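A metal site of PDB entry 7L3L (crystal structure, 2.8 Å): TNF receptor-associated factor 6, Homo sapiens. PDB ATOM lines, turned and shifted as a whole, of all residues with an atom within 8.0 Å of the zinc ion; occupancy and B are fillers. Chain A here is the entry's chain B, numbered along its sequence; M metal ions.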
ATOM      1  N   ILE A   2     -17.134 -14.077 -21.195  1.00  0.00           N
ATOM      2  CA  ILE A   2     -16.759 -15.474 -21.404  1.00  0.00           C
ATOM      3  C   ILE A   2     -15.526 -15.749 -20.560  1.00  0.00           C
ATOM      4  O   ILE A   2     -14.489 -15.081 -20.720  1.00  0.00           O
ATOM      5  CB  ILE A   2     -16.482 -15.761 -22.888  1.00  0.00           C
ATOM      6  CG1 ILE A   2     -17.489 -15.021 -23.772  1.00  0.00           C
ATOM      7  CG2 ILE A   2     -16.516 -17.250 -23.161  1.00  0.00           C
ATOM      8  CD1 ILE A   2     -16.951 -13.758 -24.423  1.00  0.00           C
ATOM      9  N   GLN A   3     -15.629 -16.708 -19.630  1.00  0.00           N
ATOM     10  CA  GLN A   3     -14.550 -16.956 -18.690  1.00  0.00           C
ATOM     11  C   GLN A   3     -13.947 -18.355 -18.819  1.00  0.00           C
ATOM     12  O   GLN A   3     -12.745 -18.460 -19.092  1.00  0.00           O
ATOM     13  CB  GLN A   3     -15.069 -16.719 -17.268  1.00  0.00           C
ATOM     14  CG  GLN A   3     -15.539 -15.305 -17.058  1.00  0.00           C
ATOM     15  CD  GLN A   3     -16.390 -15.171 -15.813  1.00  0.00           C
ATOM     16  OE1 GLN A   3     -15.880 -15.211 -14.690  1.00  0.00           O
ATOM     17  NE2 GLN A   3     -17.693 -15.021 -16.006  1.00  0.00           N
ATOM     18  N   GLY A   4     -14.719 -19.415 -18.659  1.00  0.00           N
ATOM     19  CA  GLY A   4     -14.140 -20.735 -18.621  1.00  0.00           C
ATOM     20  C   GLY A   4     -15.224 -21.802 -18.631  1.00  0.00           C
ATOM     21  O   GLY A   4     -16.390 -21.521 -18.881  1.00  0.00           O
ATOM     22  N   TYR A   5     -14.811 -23.033 -18.341  1.00  0.00           N
ATOM     23  CA  TYR A   5     -15.741 -24.169 -18.324  1.00  0.00           C
ATOM     24  C   TYR A   5     -16.306 -24.373 -16.924  1.00  0.00           C
ATOM     25  O   TYR A   5     -15.546 -24.543 -15.950  1.00  0.00           O
ATOM     26  CB  TYR A   5     -15.042 -25.438 -18.815  1.00  0.00           C
ATOM     27  CG  TYR A   5     -14.681 -25.443 -20.286  1.00  0.00           C
ATOM     28  CD1 TYR A   5     -15.676 -25.445 -21.268  1.00  0.00           C
ATOM     29  CD2 TYR A   5     -13.357 -25.449 -20.696  1.00  0.00           C
ATOM     30  CE1 TYR A   5     -15.355 -25.452 -22.614  1.00  0.00           C
ATOM     31  CE2 TYR A   5     -13.026 -25.456 -22.038  1.00  0.00           C
ATOM     32  CZ  TYR A   5     -14.034 -25.461 -22.991  1.00  0.00           C
ATOM     33  OH  TYR A   5     -13.703 -25.460 -24.330  1.00  0.00           O
ATOM     34  N   GLU A  18      -6.112 -24.925 -14.821  1.00  0.00           N
ATOM     35  CA  GLU A  18      -7.046 -23.976 -14.251  1.00  0.00           C
ATOM     36  C   GLU A  18      -6.593 -22.561 -14.560  1.00  0.00           C
ATOM     37  O   GLU A  18      -5.414 -22.235 -14.370  1.00  0.00           O
ATOM     38  CB  GLU A  18      -7.170 -24.177 -12.731  1.00  0.00           C
ATOM     39  CG  GLU A  18      -7.984 -23.119 -12.020  1.00  0.00           C
ATOM     40  CD  GLU A  18      -8.219 -23.452 -10.564  1.00  0.00           C
ATOM     41  OE1 GLU A  18      -8.763 -24.544 -10.278  1.00  0.00           O
ATOM     42  OE2 GLU A  18      -7.837 -22.635  -9.690  1.00  0.00           O
ATOM     43  N   CYS A  19      -7.515 -21.734 -15.031  1.00  0.00           N
ATOM     44  CA  CYS A  19      -7.178 -20.359 -15.388  1.00  0.00           C
ATOM     45  C   CYS A  19      -7.002 -19.513 -14.130  1.00  0.00           C
ATOM     46  O   CYS A  19      -7.926 -19.436 -13.314  1.00  0.00           O
ATOM     47  CB  CYS A  19      -8.269 -19.756 -16.266  1.00  0.00           C
ATOM     48  SG  CYS A  19      -8.096 -17.984 -16.551  1.00  0.00           S
ATOM     49  N   PRO A  20      -5.852 -18.876 -13.931  1.00  0.00           N
ATOM     50  CA  PRO A  20      -5.660 -18.043 -12.743  1.00  0.00           C
ATOM     51  C   PRO A  20      -6.568 -16.821 -12.692  1.00  0.00           C
ATOM     52  O   PRO A  20      -6.654 -16.196 -11.632  1.00  0.00           O
ATOM     53  CB  PRO A  20      -4.183 -17.643 -12.812  1.00  0.00           C
ATOM     54  CG  PRO A  20      -3.553 -18.644 -13.724  1.00  0.00           C
ATOM     55  CD  PRO A  20      -4.609 -19.004 -14.719  1.00  0.00           C
ATOM     56  N   ILE A  21      -7.218 -16.447 -13.795  1.00  0.00           N
ATOM     57  CA  ILE A  21      -8.098 -15.275 -13.778  1.00  0.00           C
ATOM     58  C   ILE A  21      -9.495 -15.688 -13.344  1.00  0.00           C
ATOM     59  O   ILE A  21      -9.969 -15.273 -12.273  1.00  0.00           O
ATOM     60  CB  ILE A  21      -8.136 -14.580 -15.145  1.00  0.00           C
ATOM     61  CG1 ILE A  21      -6.840 -13.831 -15.410  1.00  0.00           C
ATOM     62  CG2 ILE A  21      -9.319 -13.622 -15.222  1.00  0.00           C
ATOM     63  CD1 ILE A  21      -6.855 -13.020 -16.689  1.00  0.00           C
ATOM     64  N   CYS A  22     -10.159 -16.520 -14.139  1.00  0.00           N
ATOM     65  CA  CYS A  22     -11.550 -16.874 -13.890  1.00  0.00           C
ATOM     66  C   CYS A  22     -11.690 -18.099 -13.004  1.00  0.00           C
ATOM     67  O   CYS A  22     -12.824 -18.476 -12.672  1.00  0.00           O
ATOM     68  CB  CYS A  22     -12.262 -17.114 -15.221  1.00  0.00           C
ATOM     69  SG  CYS A  22     -11.679 -18.537 -16.146  1.00  0.00           S
ATOM     70  N   LEU A  23     -10.582 -18.731 -12.608  1.00  0.00           N
ATOM     71  CA  LEU A  23     -10.597 -19.887 -11.716  1.00  0.00           C
ATOM     72  C   LEU A  23     -11.440 -21.030 -12.296  1.00  0.00           C
ATOM     73  O   LEU A  23     -12.207 -21.675 -11.585  1.00  0.00           O
ATOM     74  CB  LEU A  23     -11.086 -19.505 -10.322  1.00  0.00           C
ATOM     75  CG  LEU A  23     -10.195 -18.527  -9.559  1.00  0.00           C
ATOM     76  CD1 LEU A  23     -10.687 -18.353  -8.141  1.00  0.00           C
ATOM     77  CD2 LEU A  23      -8.753 -19.016  -9.576  1.00  0.00           C
ATOM     78  N   MET A  24     -11.288 -21.275 -13.591  1.00  0.00           N
ATOM     79  CA  MET A  24     -12.017 -22.327 -14.267  1.00  0.00           C
ATOM     80  C   MET A  24     -11.133 -22.949 -15.341  1.00  0.00           C
ATOM     81  O   MET A  24     -10.058 -22.425 -15.668  1.00  0.00           O
ATOM     82  CB  MET A  24     -13.328 -21.794 -14.861  1.00  0.00           C
ATOM     83  CG  MET A  24     -14.514 -21.947 -13.924  1.00  0.00           C
ATOM     84  SD  MET A  24     -15.774 -20.669 -14.116  1.00  0.00           S
ATOM     85  CE  MET A  24     -16.578 -21.175 -15.624  1.00  0.00           C
ATOM     86  N   ALA A  25     -11.576 -24.086 -15.865  1.00  0.00           N
ATOM     87  CA  ALA A  25     -10.795 -24.797 -16.872  1.00  0.00           C
ATOM     88  C   ALA A  25     -10.632 -23.938 -18.119  1.00  0.00           C
ATOM     89  O   ALA A  25     -11.599 -23.317 -18.598  1.00  0.00           O
ATOM     90  CB  ALA A  25     -11.455 -26.124 -17.237  1.00  0.00           C
ATOM     91  N   LEU A  26      -9.410 -23.909 -18.643  1.00  0.00           N
ATOM     92  CA  LEU A  26      -9.066 -22.962 -19.694  1.00  0.00           C
ATOM     93  C   LEU A  26      -9.932 -23.166 -20.925  1.00  0.00           C
ATOM     94  O   LEU A  26     -10.126 -24.294 -21.390  1.00  0.00           O
ATOM     95  CB  LEU A  26      -7.585 -23.132 -20.060  1.00  0.00           C
ATOM     96  CG  LEU A  26      -6.608 -23.142 -18.901  1.00  0.00           C
ATOM     97  CD1 LEU A  26      -5.371 -23.929 -19.258  1.00  0.00           C
ATOM     98  CD2 LEU A  26      -6.232 -21.733 -18.533  1.00  0.00           C
ATOM     99  N   ARG A  27     -10.459 -22.063 -21.457  1.00  0.00           N
ATOM    100  CA  ARG A  27     -11.253 -22.074 -22.673  1.00  0.00           C
ATOM    101  C   ARG A  27     -10.446 -21.437 -23.786  1.00  0.00           C
ATOM    102  O   ARG A  27     -10.094 -20.245 -23.696  1.00  0.00           O
ATOM    103  CB  ARG A  27     -12.579 -21.336 -22.463  1.00  0.00           C
ATOM    104  CG  ARG A  27     -13.248 -20.935 -23.754  1.00  0.00           C
ATOM    105  CD  ARG A  27     -14.626 -20.384 -23.499  1.00  0.00           C
ATOM    106  NE  ARG A  27     -15.608 -21.463 -23.469  1.00  0.00           N
ATOM    107  CZ  ARG A  27     -16.373 -21.728 -22.427  1.00  0.00           C
ATOM    108  NH1 ARG A  27     -16.277 -20.991 -21.328  1.00  0.00           N
ATOM    109  NH2 ARG A  27     -17.258 -22.722 -22.479  1.00  0.00           N
ATOM    110  N   ARG A  37      -0.663 -20.297 -18.205  1.00  0.00           N
ATOM    111  CA  ARG A  37      -1.787 -20.511 -19.093  1.00  0.00           C
ATOM    112  C   ARG A  37      -2.997 -19.720 -18.616  1.00  0.00           C
ATOM    113  O   ARG A  37      -3.256 -19.612 -17.420  1.00  0.00           O
ATOM    114  CB  ARG A  37      -2.144 -22.008 -19.159  1.00  0.00           C
ATOM    115  CG  ARG A  37      -0.959 -22.914 -19.475  1.00  0.00           C
ATOM    116  CD  ARG A  37      -1.389 -24.371 -19.616  1.00  0.00           C
ATOM    117  NE  ARG A  37      -0.310 -25.225 -20.087  1.00  0.00           N
ATOM    118  CZ  ARG A  37       0.372 -26.083 -19.323  1.00  0.00           C
ATOM    119  NH1 ARG A  37       0.070 -26.192 -18.033  1.00  0.00           N
ATOM    120  NH2 ARG A  37       1.347 -26.811 -19.844  1.00  0.00           N
ATOM    121  N   PHE A  38      -3.734 -19.152 -19.575  1.00  0.00           N
ATOM    122  CA  PHE A  38      -4.979 -18.437 -19.303  1.00  0.00           C
ATOM    123  C   PHE A  38      -5.983 -18.824 -20.382  1.00  0.00           C
ATOM    124  O   PHE A  38      -5.639 -19.450 -21.384  1.00  0.00           O
ATOM    125  CB  PHE A  38      -4.793 -16.914 -19.291  1.00  0.00           C
ATOM    126  CG  PHE A  38      -3.760 -16.420 -18.304  1.00  0.00           C
ATOM    127  CD1 PHE A  38      -2.421 -16.355 -18.650  1.00  0.00           C
ATOM    128  CD2 PHE A  38      -4.143 -15.974 -17.046  1.00  0.00           C
ATOM    129  CE1 PHE A  38      -1.475 -15.882 -17.749  1.00  0.00           C
ATOM    130  CE2 PHE A  38      -3.202 -15.505 -16.136  1.00  0.00           C
ATOM    131  CZ  PHE A  38      -1.871 -15.457 -16.494  1.00  0.00           C
ATOM    132  N   CYS A  39      -7.231 -18.430 -20.176  1.00  0.00           N
ATOM    133  CA  CYS A  39      -8.177 -18.441 -21.283  1.00  0.00           C
ATOM    134  C   CYS A  39      -7.856 -17.276 -22.209  1.00  0.00           C
ATOM    135  O   CYS A  39      -7.353 -16.244 -21.789  1.00  0.00           O
ATOM    136  CB  CYS A  39      -9.607 -18.325 -20.764  1.00  0.00           C
ATOM    137  SG  CYS A  39      -9.932 -19.285 -19.280  1.00  0.00           S
ATOM    138  N   LYS A  40      -8.143 -17.468 -23.502  1.00  0.00           N
ATOM    139  CA  LYS A  40      -7.874 -16.401 -24.462  1.00  0.00           C
ATOM    140  C   LYS A  40      -8.678 -15.147 -24.121  1.00  0.00           C
ATOM    141  O   LYS A  40      -8.146 -14.036 -24.153  1.00  0.00           O
ATOM    142  CB  LYS A  40      -8.188 -16.857 -25.877  1.00  0.00           C
ATOM    143  CG  LYS A  40      -7.847 -15.806 -26.942  1.00  0.00           C
ATOM    144  CD  LYS A  40      -7.869 -16.395 -28.344  1.00  0.00           C
ATOM    145  CE  LYS A  40      -9.221 -17.025 -28.658  1.00  0.00           C
ATOM    146  NZ  LYS A  40      -9.156 -17.937 -29.836  1.00  0.00           N
ATOM    147  N   ALA A  41      -9.956 -15.320 -23.773  1.00  0.00           N
ATOM    148  CA  ALA A  41     -10.794 -14.167 -23.459  1.00  0.00           C
ATOM    149  C   ALA A  41     -10.339 -13.488 -22.162  1.00  0.00           C
ATOM    150  O   ALA A  41     -10.256 -12.257 -22.094  1.00  0.00           O
ATOM    151  CB  ALA A  41     -12.254 -14.590 -23.357  1.00  0.00           C
ATOM    152  N   CYS A  42     -10.049 -14.275 -21.128  1.00  0.00           N
ATOM    153  CA  CYS A  42      -9.708 -13.703 -19.826  1.00  0.00           C
ATOM    154  C   CYS A  42      -8.442 -12.852 -19.903  1.00  0.00           C
ATOM    155  O   CYS A  42      -8.392 -11.744 -19.358  1.00  0.00           O
ATOM    156  CB  CYS A  42      -9.548 -14.807 -18.782  1.00  0.00           C
ATOM    157  SG  CYS A  42     -11.071 -15.724 -18.436  1.00  0.00           S
ATOM    158  N   ILE A  43      -7.410 -13.356 -20.580  1.00  0.00           N
ATOM    159  CA  ILE A  43      -6.116 -12.695 -20.518  1.00  0.00           C
ATOM    160  C   ILE A  43      -6.121 -11.423 -21.353  1.00  0.00           C
ATOM    161  O   ILE A  43      -5.523 -10.408 -20.958  1.00  0.00           O
ATOM    162  CB  ILE A  43      -4.991 -13.663 -20.949  1.00  0.00           C
ATOM    163  CG1 ILE A  43      -3.625 -12.975 -20.841  1.00  0.00           C
ATOM    164  CG2 ILE A  43      -5.216 -14.172 -22.360  1.00  0.00           C
ATOM    165  CD1 ILE A  43      -3.342 -12.372 -19.491  1.00  0.00           C
HETATM  166 ZN    ZN M   1     -10.189 -17.713 -17.659  1.00  0.00          ZN
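SG of Cys 39 is bound to the zinc ion (2.3 Å). The zinc ion is bound by SG of Cys 22 (2.3 Å). The zinc ion is bound by SG of Cys 42, 2.3 Å away. SG of Cys 19 binds the zinc ion, at 2.4 Å.
The side-chain sulfur of Cys 39 lies close to the backbone carbonyl oxygen of Gln 3 (2.9 Å). The side-chain sulfur (SG) of Cys 19 lies close to the backbone NH (N) of Ile 21, at 3.3 Å. The backbone carbonyl oxygen (O) of Met 24 lies within hydrogen-bond range of the backbone NH (N) of Cys 19 (2.7 Å). SG of Cys 22 lies close to N of Met 24 (3.8 Å). SG of Cys 22 sits close to O of Gln 3 (3.1 Å). SG of Cys 42 lies close to O of Gln 3 (3.3 Å). SG of Cys 39 lies close to N of Arg 27 (3.6 Å).
Gln 3 touches the zinc ion. Of the 21 residues printed, 5 come within 4 Å of the zinc ion. Along chain A the residues within 4 Å of the zinc ion span positions 3 to 42.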
